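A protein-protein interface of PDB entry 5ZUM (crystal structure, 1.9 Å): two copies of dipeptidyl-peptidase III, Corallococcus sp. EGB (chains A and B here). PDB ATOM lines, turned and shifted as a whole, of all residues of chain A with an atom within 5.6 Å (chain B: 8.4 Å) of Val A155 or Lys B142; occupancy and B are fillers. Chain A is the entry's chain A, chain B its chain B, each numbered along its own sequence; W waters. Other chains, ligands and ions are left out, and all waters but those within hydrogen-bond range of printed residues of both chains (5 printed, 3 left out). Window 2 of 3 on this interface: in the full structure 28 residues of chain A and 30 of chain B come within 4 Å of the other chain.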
ATOM      1  N   VAL A 151      15.548  15.292   4.257  1.00  0.00           N
ATOM      2  CA  VAL A 151      15.107  13.940   4.598  1.00  0.00           C
ATOM      3  C   VAL A 151      13.950  13.555   3.681  1.00  0.00           C
ATOM      4  O   VAL A 151      12.943  14.240   3.646  1.00  0.00           O
ATOM      5  CB  VAL A 151      14.644  13.867   6.068  1.00  0.00           C
ATOM      6  CG1 VAL A 151      14.342  12.426   6.493  1.00  0.00           C
ATOM      7  CG2 VAL A 151      15.690  14.461   7.005  1.00  0.00           C
ATOM      8  N   PRO A 152      14.096  12.483   2.902  1.00  0.00           N
ATOM      9  CA  PRO A 152      12.930  12.004   2.123  1.00  0.00           C
ATOM     10  C   PRO A 152      11.707  11.749   2.982  1.00  0.00           C
ATOM     11  O   PRO A 152      11.808  11.108   4.051  1.00  0.00           O
ATOM     12  CB  PRO A 152      13.413  10.691   1.518  1.00  0.00           C
ATOM     13  CG  PRO A 152      14.892  10.605   1.755  1.00  0.00           C
ATOM     14  CD  PRO A 152      15.282  11.625   2.784  1.00  0.00           C
ATOM     15  N   TYR A 153      10.527  12.046   2.446  1.00  0.00           N
ATOM     16  CA  TYR A 153       9.295  11.663   3.101  1.00  0.00           C
ATOM     17  C   TYR A 153       9.237  10.173   3.461  1.00  0.00           C
ATOM     18  O   TYR A 153       8.686   9.791   4.502  1.00  0.00           O
ATOM     19  CB  TYR A 153       8.121  12.005   2.188  1.00  0.00           C
ATOM     20  CG  TYR A 153       7.682  13.470   2.276  1.00  0.00           C
ATOM     21  CD1 TYR A 153       8.499  14.473   2.809  1.00  0.00           C
ATOM     22  CD2 TYR A 153       6.432  13.831   1.796  1.00  0.00           C
ATOM     23  CE1 TYR A 153       8.013  15.782   2.958  1.00  0.00           C
ATOM     24  CE2 TYR A 153       5.957  15.118   1.915  1.00  0.00           C
ATOM     25  CZ  TYR A 153       6.748  16.101   2.480  1.00  0.00           C
ATOM     26  OH  TYR A 153       6.166  17.356   2.638  1.00  0.00           O
ATOM     27  N   SER A 154       9.869   9.337   2.636  1.00  0.00           N
ATOM     28  CA  SER A 154       9.782   7.895   2.794  1.00  0.00           C
ATOM     29  C   SER A 154      10.541   7.457   4.059  1.00  0.00           C
ATOM     30  O   SER A 154      10.252   6.428   4.649  1.00  0.00           O
ATOM     31  CB  SER A 154      10.414   7.224   1.585  1.00  0.00           C
ATOM     32  OG  SER A 154      11.718   7.732   1.371  1.00  0.00           O
ATOM     33  N   VAL A 155      11.489   8.264   4.474  1.00  0.00           N
ATOM     34  CA  VAL A 155      12.241   8.061   5.715  1.00  0.00           C
ATOM     35  C   VAL A 155      11.605   8.796   6.912  1.00  0.00           C
ATOM     36  O   VAL A 155      11.254   8.176   7.939  1.00  0.00           O
ATOM     37  CB  VAL A 155      13.698   8.478   5.461  1.00  0.00           C
ATOM     38  CG1 VAL A 155      14.452   8.611   6.780  1.00  0.00           C
ATOM     39  CG2 VAL A 155      14.344   7.464   4.499  1.00  0.00           C
ATOM     40  N   GLU A 156      11.244  10.050   6.678  1.00  0.00           N
ATOM     41  CA  GLU A 156      10.625  10.910   7.688  1.00  0.00           C
ATOM     42  C   GLU A 156       9.357  10.295   8.271  1.00  0.00           C
ATOM     43  O   GLU A 156       9.165  10.333   9.495  1.00  0.00           O
ATOM     44  CB  GLU A 156      10.325  12.284   7.089  1.00  0.00           C
ATOM     45  CG  GLU A 156       9.522  13.232   7.969  1.00  0.00           C
ATOM     46  CD  GLU A 156      10.353  13.937   9.033  1.00  0.00           C
ATOM     47  OE1 GLU A 156      11.418  14.517   8.732  1.00  0.00           O
ATOM     48  OE2 GLU A 156       9.804  14.135  10.114  1.00  0.00           O
ATOM     49  N   TYR A 157       8.467   9.794   7.411  1.00  0.00           N
ATOM     50  CA  TYR A 157       7.208   9.193   7.826  1.00  0.00           C
ATOM     51  C   TYR A 157       7.146   7.651   7.643  1.00  0.00           C
ATOM     52  O   TYR A 157       6.116   7.084   7.451  1.00  0.00           O
ATOM     53  CB  TYR A 157       6.065   9.858   7.089  1.00  0.00           C
ATOM     54  CG  TYR A 157       6.130  11.361   7.038  1.00  0.00           C
ATOM     55  CD1 TYR A 157       5.896  12.136   8.153  1.00  0.00           C
ATOM     56  CD2 TYR A 157       6.429  11.996   5.881  1.00  0.00           C
ATOM     57  CE1 TYR A 157       5.945  13.495   8.105  1.00  0.00           C
ATOM     58  CE2 TYR A 157       6.520  13.347   5.818  1.00  0.00           C
ATOM     59  CZ  TYR A 157       6.267  14.116   6.923  1.00  0.00           C
ATOM     60  OH  TYR A 157       6.348  15.448   6.817  1.00  0.00           O
ATOM     61  N   GLN A 158       8.303   7.037   7.737  1.00  0.00           N
ATOM     62  CA  GLN A 158       8.468   5.624   7.446  1.00  0.00           C
ATOM     63  C   GLN A 158       7.479   4.610   8.075  1.00  0.00           C
ATOM     64  O   GLN A 158       6.871   3.844   7.381  1.00  0.00           O
ATOM     65  CB  GLN A 158       9.925   5.189   7.602  1.00  0.00           C
ATOM     66  CG  GLN A 158      10.133   3.760   7.159  1.00  0.00           C
ATOM     67  CD  GLN A 158      11.474   3.455   6.516  1.00  0.00           C
ATOM     68  OE1 GLN A 158      12.084   2.483   6.821  1.00  0.00           O
ATOM     69  NE2 GLN A 158      11.875   4.262   5.620  1.00  0.00           N
ATOM     70  N   GLY A 159       7.329   4.657   9.389  1.00  0.00           N
ATOM     71  CA  GLY A 159       6.453   3.731  10.072  1.00  0.00           C
ATOM     72  C   GLY A 159       5.043   3.746   9.572  1.00  0.00           C
ATOM     73  O   GLY A 159       4.499   2.780   9.160  1.00  0.00           O
ATOM     74  N   LEU A 192       7.583   4.098  -0.023  1.00  0.00           N
ATOM     75  CA  LEU A 192       8.925   3.751   0.445  1.00  0.00           C
ATOM     76  C   LEU A 192      10.089   4.151  -0.472  1.00  0.00           C
ATOM     77  O   LEU A 192      11.194   4.398   0.003  1.00  0.00           O
ATOM     78  CB  LEU A 192       8.984   2.277   0.774  1.00  0.00           C
ATOM     79  CG  LEU A 192       8.697   1.961   2.244  1.00  0.00           C
ATOM     80  CD1 LEU A 192       9.884   2.445   3.085  1.00  0.00           C
ATOM     81  CD2 LEU A 192       7.390   2.571   2.729  1.00  0.00           C
ATOM     82  N   ASN A 194      10.024   6.884  -2.383  1.00  0.00           N
ATOM     83  CA  ASN A 194       9.916   8.342  -2.458  1.00  0.00           C
ATOM     84  C   ASN A 194       9.912   8.863  -3.888  1.00  0.00           C
ATOM     85  O   ASN A 194      10.047  10.065  -4.092  1.00  0.00           O
ATOM     86  CB  ASN A 194      11.031   9.054  -1.699  1.00  0.00           C
ATOM     87  CG  ASN A 194      10.567  10.341  -1.055  1.00  0.00           C
ATOM     88  OD1 ASN A 194       9.583  10.341  -0.295  1.00  0.00           O
ATOM     89  ND2 ASN A 194      11.311  11.429  -1.285  1.00  0.00           N
ATOM     90  N   ASN B 107       8.816   1.022  16.666  1.00  0.00           N
ATOM     91  CA  ASN B 107       8.954   1.825  15.439  1.00  0.00           C
ATOM     92  C   ASN B 107      10.378   2.362  15.315  1.00  0.00           C
ATOM     93  O   ASN B 107      10.597   3.479  14.870  1.00  0.00           O
ATOM     94  CB  ASN B 107       7.924   2.962  15.454  1.00  0.00           C
ATOM     95  CG  ASN B 107       7.902   3.798  14.162  1.00  0.00           C
ATOM     96  OD1 ASN B 107       7.595   4.998  14.200  1.00  0.00           O
ATOM     97  ND2 ASN B 107       8.233   3.194  13.043  1.00  0.00           N
ATOM     98  N   PHE B 108      11.346   1.529  15.662  1.00  0.00           N
ATOM     99  CA  PHE B 108      12.739   1.906  15.662  1.00  0.00           C
ATOM    100  C   PHE B 108      13.477   1.449  14.416  1.00  0.00           C
ATOM    101  O   PHE B 108      14.592   1.900  14.180  1.00  0.00           O
ATOM    102  CB  PHE B 108      13.443   1.297  16.853  1.00  0.00           C
ATOM    103  CG  PHE B 108      12.884   1.686  18.195  1.00  0.00           C
ATOM    104  CD1 PHE B 108      13.227   2.899  18.776  1.00  0.00           C
ATOM    105  CD2 PHE B 108      12.240   0.744  18.976  1.00  0.00           C
ATOM    106  CE1 PHE B 108      12.808   3.222  20.039  1.00  0.00           C
ATOM    107  CE2 PHE B 108      11.827   1.053  20.248  1.00  0.00           C
ATOM    108  CZ  PHE B 108      12.068   2.308  20.768  1.00  0.00           C
ATOM    109  N   TYR B 109      12.886   0.509  13.670  1.00  0.00           N
ATOM    110  CA  TYR B 109      13.578  -0.201  12.602  1.00  0.00           C
ATOM    111  C   TYR B 109      12.875  -0.076  11.250  1.00  0.00           C
ATOM    112  O   TYR B 109      11.833   0.559  11.168  1.00  0.00           O
ATOM    113  CB  TYR B 109      13.831  -1.657  13.002  1.00  0.00           C
ATOM    114  CG  TYR B 109      14.778  -1.803  14.184  1.00  0.00           C
ATOM    115  CD1 TYR B 109      16.150  -1.643  14.033  1.00  0.00           C
ATOM    116  CD2 TYR B 109      14.283  -2.016  15.465  1.00  0.00           C
ATOM    117  CE1 TYR B 109      17.028  -1.794  15.107  1.00  0.00           C
ATOM    118  CE2 TYR B 109      15.136  -2.085  16.565  1.00  0.00           C
ATOM    119  CZ  TYR B 109      16.504  -2.000  16.379  1.00  0.00           C
ATOM    120  OH  TYR B 109      17.362  -2.061  17.462  1.00  0.00           O
ATOM    121  N   PRO B 110      13.501  -0.592  10.159  1.00  0.00           N
ATOM    122  CA  PRO B 110      12.937  -0.322   8.839  1.00  0.00           C
ATOM    123  C   PRO B 110      11.566  -0.921   8.632  1.00  0.00           C
ATOM    124  O   PRO B 110      11.279  -2.062   9.061  1.00  0.00           O
ATOM    125  CB  PRO B 110      13.972  -0.907   7.862  1.00  0.00           C
ATOM    126  CG  PRO B 110      15.258  -0.899   8.627  1.00  0.00           C
ATOM    127  CD  PRO B 110      14.844  -1.191  10.058  1.00  0.00           C
ATOM    128  N   ALA B 111      10.738  -0.183   7.909  1.00  0.00           N
ATOM    129  CA  ALA B 111       9.458  -0.721   7.505  1.00  0.00           C
ATOM    130  C   ALA B 111       9.633  -2.037   6.721  1.00  0.00           C
ATOM    131  O   ALA B 111      10.436  -2.139   5.806  1.00  0.00           O
ATOM    132  CB  ALA B 111       8.646   0.295   6.724  1.00  0.00           C
ATOM    133  N   GLY B 112       8.959  -3.072   7.199  1.00  0.00           N
ATOM    134  CA  GLY B 112       9.000  -4.385   6.547  1.00  0.00           C
ATOM    135  C   GLY B 112      10.146  -5.269   6.993  1.00  0.00           C
ATOM    136  O   GLY B 112      10.249  -6.429   6.549  1.00  0.00           O
ATOM    137  N   ALA B 113      11.046  -4.740   7.817  1.00  0.00           N
ATOM    138  CA  ALA B 113      12.247  -5.495   8.176  1.00  0.00           C
ATOM    139  C   ALA B 113      11.931  -6.662   9.126  1.00  0.00           C
ATOM    140  O   ALA B 113      10.896  -6.682   9.809  1.00  0.00           O
ATOM    141  CB  ALA B 113      13.267  -4.587   8.809  1.00  0.00           C
ATOM    142  N   GLU B 117      17.219  -9.625   9.094  1.00  0.00           N
ATOM    143  CA  GLU B 117      17.661  -8.661   8.078  1.00  0.00           C
ATOM    144  C   GLU B 117      18.480  -7.521   8.664  1.00  0.00           C
ATOM    145  O   GLU B 117      19.560  -7.164   8.148  1.00  0.00           O
ATOM    146  CB  GLU B 117      16.474  -8.081   7.327  1.00  0.00           C
ATOM    147  CG  GLU B 117      15.960  -8.968   6.214  1.00  0.00           C
ATOM    148  CD  GLU B 117      14.592  -8.513   5.741  1.00  0.00           C
ATOM    149  OE1 GLU B 117      14.051  -7.546   6.321  1.00  0.00           O
ATOM    150  OE2 GLU B 117      14.075  -9.088   4.766  1.00  0.00           O
ATOM    151  N   THR B 139      17.525   5.795  14.947  1.00  0.00           N
ATOM    152  CA  THR B 139      16.645   4.839  14.353  1.00  0.00           C
ATOM    153  C   THR B 139      17.337   4.248  13.136  1.00  0.00           C
ATOM    154  O   THR B 139      18.312   4.830  12.595  1.00  0.00           O
ATOM    155  CB  THR B 139      15.288   5.438  13.955  1.00  0.00           C
ATOM    156  OG1 THR B 139      15.469   6.573  13.092  1.00  0.00           O
ATOM    157  CG2 THR B 139      14.483   5.866  15.150  1.00  0.00           C
ATOM    158  N   VAL B 140      16.737   3.164  12.651  1.00  0.00           N
ATOM    159  CA  VAL B 140      17.126   2.543  11.386  1.00  0.00           C
ATOM    160  C   VAL B 140      15.976   2.477  10.406  1.00  0.00           C
ATOM    161  O   VAL B 140      14.910   1.977  10.717  1.00  0.00           O
ATOM    162  CB  VAL B 140      17.641   1.115  11.635  1.00  0.00           C
ATOM    163  CG1 VAL B 140      18.214   0.517  10.367  1.00  0.00           C
ATOM    164  CG2 VAL B 140      18.711   1.118  12.701  1.00  0.00           C
ATOM    165  N   ARG B 141      16.188   3.029   9.203  1.00  0.00           N
ATOM    166  CA  ARG B 141      15.159   3.195   8.192  1.00  0.00           C
ATOM    167  C   ARG B 141      15.675   2.624   6.864  1.00  0.00           C
ATOM    168  O   ARG B 141      16.874   2.640   6.618  1.00  0.00           O
ATOM    169  CB  ARG B 141      14.903   4.697   7.947  1.00  0.00           C
ATOM    170  CG  ARG B 141      14.101   5.523   8.964  1.00  0.00           C
ATOM    171  CD  ARG B 141      13.828   4.841  10.259  1.00  0.00           C
ATOM    172  NE  ARG B 141      12.823   5.435  11.147  1.00  0.00           N
ATOM    173  CZ  ARG B 141      12.010   4.683  11.882  1.00  0.00           C
ATOM    174  NH1 ARG B 141      12.083   3.374  11.783  1.00  0.00           N
ATOM    175  NH2 ARG B 141      11.099   5.209  12.697  1.00  0.00           N
ATOM    176  N   LYS B 142      14.757   2.204   6.003  1.00  0.00           N
ATOM    177  CA  LYS B 142      15.084   1.883   4.601  1.00  0.00           C
ATOM    178  C   LYS B 142      15.093   3.184   3.785  1.00  0.00           C
ATOM    179  O   LYS B 142      14.169   3.974   3.874  1.00  0.00           O
ATOM    180  CB  LYS B 142      14.026   0.882   4.117  1.00  0.00           C
ATOM    181  CG  LYS B 142      14.213   0.261   2.752  1.00  0.00           C
ATOM    182  CD  LYS B 142      12.974  -0.561   2.396  1.00  0.00           C
ATOM    183  CE  LYS B 142      13.210  -2.064   2.498  1.00  0.00           C
ATOM    184  NZ  LYS B 142      13.270  -2.717   1.155  1.00  0.00           N
ATOM    185  N   GLY B 143      16.216   3.471   3.124  1.00  0.00           N
ATOM    186  CA  GLY B 143      16.358   4.672   2.292  1.00  0.00           C
ATOM    187  C   GLY B 143      15.743   4.480   0.918  1.00  0.00           C
ATOM    188  O   GLY B 143      15.262   3.386   0.588  1.00  0.00           O
ATOM    189  N   PRO B 144      15.762   5.531   0.100  1.00  0.00           N
ATOM    190  CA  PRO B 144      15.060   5.425  -1.168  1.00  0.00           C
ATOM    191  C   PRO B 144      15.623   4.351  -2.090  1.00  0.00           C
ATOM    192  O   PRO B 144      14.857   3.685  -2.752  1.00  0.00           O
ATOM    193  CB  PRO B 144      15.239   6.821  -1.787  1.00  0.00           C
ATOM    194  CG  PRO B 144      15.327   7.727  -0.602  1.00  0.00           C
ATOM    195  CD  PRO B 144      16.002   6.933   0.484  1.00  0.00           C
ATOM    196  N   ASP B 145      16.933   4.119  -2.041  1.00  0.00           N
ATOM    197  CA  ASP B 145      17.549   3.070  -2.854  1.00  0.00           C
ATOM    198  C   ASP B 145      17.313   1.663  -2.284  1.00  0.00           C
ATOM    199  O   ASP B 145      17.811   0.675  -2.820  1.00  0.00           O
ATOM    200  CB  ASP B 145      19.036   3.342  -3.008  1.00  0.00           C
ATOM    201  CG  ASP B 145      19.761   3.335  -1.691  1.00  0.00           C
ATOM    202  OD1 ASP B 145      19.143   2.997  -0.651  1.00  0.00           O
ATOM    203  OD2 ASP B 145      20.942   3.707  -1.692  1.00  0.00           O
ATOM    204  N   GLY B 146      16.535   1.567  -1.208  1.00  0.00           N
ATOM    205  CA  GLY B 146      16.181   0.293  -0.636  1.00  0.00           C
ATOM    206  C   GLY B 146      17.111  -0.208   0.456  1.00  0.00           C
ATOM    207  O   GLY B 146      16.835  -1.227   1.081  1.00  0.00           O
ATOM    208  N   LYS B 147      18.228   0.460   0.690  1.00  0.00           N
ATOM    209  CA  LYS B 147      19.173  -0.025   1.696  1.00  0.00           C
ATOM    210  C   LYS B 147      18.949   0.655   3.046  1.00  0.00           C
ATOM    211  O   LYS B 147      18.335   1.712   3.108  1.00  0.00           O
ATOM    212  CB  LYS B 147      20.601   0.183   1.209  1.00  0.00           C
ATOM    213  CG  LYS B 147      20.884  -0.689  -0.020  1.00  0.00           C
ATOM    214  CD  LYS B 147      22.364  -0.782  -0.395  1.00  0.00           C
ATOM    215  CE  LYS B 147      22.646  -1.964  -1.326  1.00  0.00           C
ATOM    216  NZ  LYS B 147      21.763  -1.995  -2.529  1.00  0.00           N
ATOM    217  N   PHE B 148      19.453   0.060   4.118  1.00  0.00           N
ATOM    218  CA  PHE B 148      19.124   0.545   5.451  1.00  0.00           C
ATOM    219  C   PHE B 148      20.068   1.701   5.740  1.00  0.00           C
ATOM    220  O   PHE B 148      21.168   1.786   5.188  1.00  0.00           O
ATOM    221  CB  PHE B 148      19.275  -0.538   6.526  1.00  0.00           C
ATOM    222  CG  PHE B 148      18.294  -1.683   6.438  1.00  0.00           C
ATOM    223  CD1 PHE B 148      17.166  -1.642   5.633  1.00  0.00           C
ATOM    224  CD2 PHE B 148      18.460  -2.782   7.272  1.00  0.00           C
ATOM    225  CE1 PHE B 148      16.290  -2.726   5.592  1.00  0.00           C
ATOM    226  CE2 PHE B 148      17.547  -3.831   7.292  1.00  0.00           C
ATOM    227  CZ  PHE B 148      16.485  -3.821   6.414  1.00  0.00           C
ATOM    228  N   LEU B 149      19.598   2.652   6.524  1.00  0.00           N
ATOM    229  CA  LEU B 149      20.421   3.770   6.928  1.00  0.00           C
ATOM    230  C   LEU B 149      20.076   4.156   8.358  1.00  0.00           C
ATOM    231  O   LEU B 149      19.022   3.775   8.846  1.00  0.00           O
ATOM    232  CB  LEU B 149      20.240   4.952   5.963  1.00  0.00           C
ATOM    233  CG  LEU B 149      18.851   5.553   5.761  1.00  0.00           C
ATOM    234  CD1 LEU B 149      18.575   6.646   6.778  1.00  0.00           C
ATOM    235  CD2 LEU B 149      18.715   6.151   4.371  1.00  0.00           C
ATOM    236  N   THR B 150      20.990   4.881   9.003  1.00  0.00           N
ATOM    237  CA  THR B 150      20.877   5.308  10.389  1.00  0.00           C
ATOM    238  C   THR B 150      20.347   6.743  10.444  1.00  0.00           C
ATOM    239  O   THR B 150      20.745   7.578   9.642  1.00  0.00           O
ATOM    240  CB  THR B 150      22.274   5.216  11.034  1.00  0.00           C
ATOM    241  OG1 THR B 150      22.721   3.850  10.983  1.00  0.00           O
ATOM    242  CG2 THR B 150      22.252   5.620  12.440  1.00  0.00           C
ATOM    243  N   VAL B 151      19.341   7.014  11.269  1.00  0.00           N
ATOM    244  CA  VAL B 151      18.861   8.364  11.451  1.00  0.00           C
ATOM    245  C   VAL B 151      19.052   8.799  12.910  1.00  0.00           C
ATOM    246  O   VAL B 151      18.561   8.125  13.816  1.00  0.00           O
ATOM    247  CB  VAL B 151      17.391   8.479  11.030  1.00  0.00           C
ATOM    248  CG1 VAL B 151      16.894   9.904  11.151  1.00  0.00           C
ATOM    249  CG2 VAL B 151      17.213   7.998   9.579  1.00  0.00           C
ATOM    250  N   PRO B 152      19.752   9.920  13.148  1.00  0.00           N
ATOM    251  CA  PRO B 152      19.880  10.408  14.529  1.00  0.00           C
ATOM    252  C   PRO B 152      18.535  10.821  15.101  1.00  0.00           C
ATOM    253  O   PRO B 152      17.689  11.328  14.354  1.00  0.00           O
ATOM    254  CB  PRO B 152      20.809  11.630  14.387  1.00  0.00           C
ATOM    255  CG  PRO B 152      21.396  11.531  13.009  1.00  0.00           C
ATOM    256  CD  PRO B 152      20.377  10.848  12.175  1.00  0.00           C
ATOM    257  N   VAL B 155      17.188  14.227  14.459  1.00  0.00           N
ATOM    258  CA  VAL B 155      16.573  14.409  13.122  1.00  0.00           C
ATOM    259  C   VAL B 155      15.214  13.724  13.019  1.00  0.00           C
ATOM    260  O   VAL B 155      14.193  14.337  12.677  1.00  0.00           O
ATOM    261  CB  VAL B 155      17.514  13.879  12.033  1.00  0.00           C
ATOM    262  CG1 VAL B 155      16.792  13.854  10.691  1.00  0.00           C
ATOM    263  CG2 VAL B 155      18.807  14.693  12.024  1.00  0.00           C
ATOM    264  N   GLU B 156      15.136  12.222  13.345  1.00  0.00           N
ATOM    265  CA  GLU B 156      13.884  11.492  13.461  1.00  0.00           C
ATOM    266  C   GLU B 156      12.736  12.342  14.017  1.00  0.00           C
ATOM    267  O   GLU B 156      11.684  12.288  13.514  1.00  0.00           O
ATOM    268  CB  GLU B 156      14.080  10.258  14.342  1.00  0.00           C
ATOM    269  CG  GLU B 156      12.843   9.382  14.470  1.00  0.00           C
ATOM    270  CD  GLU B 156      12.439   8.752  13.151  1.00  0.00           C
ATOM    271  OE1 GLU B 156      13.328   8.253  12.431  1.00  0.00           O
ATOM    272  OE2 GLU B 156      11.231   8.758  12.834  1.00  0.00           O
HETATM  273  O   HOH W   1      13.567  13.492  10.040  1.00  0.00           O
HETATM  274  O   HOH W   2      13.307   9.481  10.058  1.00  0.00           O
HETATM  275  O   HOH W   3       8.002   6.449  11.436  1.00  0.00           O
HETATM  276  O   HOH W   4      13.086   1.953   0.018  1.00  0.00           O
HETATM  277  O   HOH W   5      11.285  11.133  11.087  1.00  0.00           O
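Of the 11 printed residues of chain A, 5 touch a printed residue of chain B. Printed residues of chain A that touch a printed residue of chain B: Val A151, Pro A152, Val A155, Gln A158 and Gly A159. Hydrophobic or aromatic side chains of chain A that line the printed part of chain B: Val A151, Pro A152 and Val A155. Of the 24 printed residues of chain B, 8 touch a printed residue of chain A. Printed residues of chain B that touch a printed residue of chain A: Asn B107, Pro B110, Ala B111, Arg B141, Lys B142, Pro B144, Val B151 and Val B155. Hydrophobic or aromatic side chains of chain B within 4 Å of the printed part of chain A: Ala B111, Pro B144, Val B151 and Val B155.
Val B155 touches Val A151 (CG1 to CG2, 3.9 Å). Pro A152 touches Pro B144 (CG to CG, 3.7 Å). Val A155 touches Arg B141. Val A155 touches Lys B142 (CG2 to O, 3.5 Å). CG1 of Val A155 touches CG2 of Val B151 (3.98 Å). Gln A158 touches Pro B110 (OE1 to CA, 3.6 Å). Arg B141 touches Gln A158. CA of Gly A159 touches ND2 of Asn B107, 3.5 Å away.
The backbone carbonyl oxygen of Ser A154 is in hydrogen-bond range of the side-chain amide nitrogen of Gln A158, 2.9 Å away. OG1 of Thr B139 lies within hydrogen-bond range of NE of Arg B141 (3.5 Å). NH1 of Arg B141 is in hydrogen-bond range of O of Tyr B109 (2.9 Å). The guanidinium group (NH2) of Arg B141 sits at hydrogen-bond distance from the backbone carbonyl oxygen (O) of Asn B107. N of Leu B149 is in hydrogen-bond range of O of Arg B141 (2.7 Å). The guanidinium group of Arg B141 lies within salt-bridge range of the side-chain carboxylate of Glu B156.
Water W4 bridges O of Gly B143 and O of Leu A192. Water W2 lies within hydrogen-bond range of the side-chain carboxylate (OE1) of Glu B156 (2.7 Å) and the backbone carbonyl oxygen (O) of Val A155 (3.2 Å). Water W1 lies within hydrogen-bond range of OE1 of Glu A156 (2.7 Å) and O of Val B155 (2.8 Å). Water W5 lies within hydrogen-bond range of O of Glu B156 (2.7 Å) and O of Glu A156 (2.8 Å). Water W3 bridges N of Gly A159 (2.8 Å) and OD1 of Asn B107 (3.1 Å).
The backbone NH of Ala B111 lies within hydrogen-bond range of the side-chain amide oxygen of Gln A158, at 3.2 Å. The side-chain amide oxygen (OE1) of Gln A158 is in hydrogen-bond range of the backbone NH (N) of Lys B142, 2.8 Å away.
Val A151 touches Val B155, and with the chains exchanged Val A155 touches Val B151. 4 positions are printed for both chains. Of the 10 pairs that touch across the chains among the printed residues, 2 have their exchanged pair printed and touching as well.
Of chain A, only Val A155 and Gln A158 come within 4 Å of Lys B142. No residue of chain B comes within 4 Å of Ser A154. Printed residues of chain A within 4 Å of Asn B107: Gly A159. Of the printed residues of chain A, Arg B141 touches Val A155 (3.8 Å) and Gln A158 (3.4 Å). Glu B117 touches none of the printed residues of chain A. Asp B145 touches none of the printed residues of chain A.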
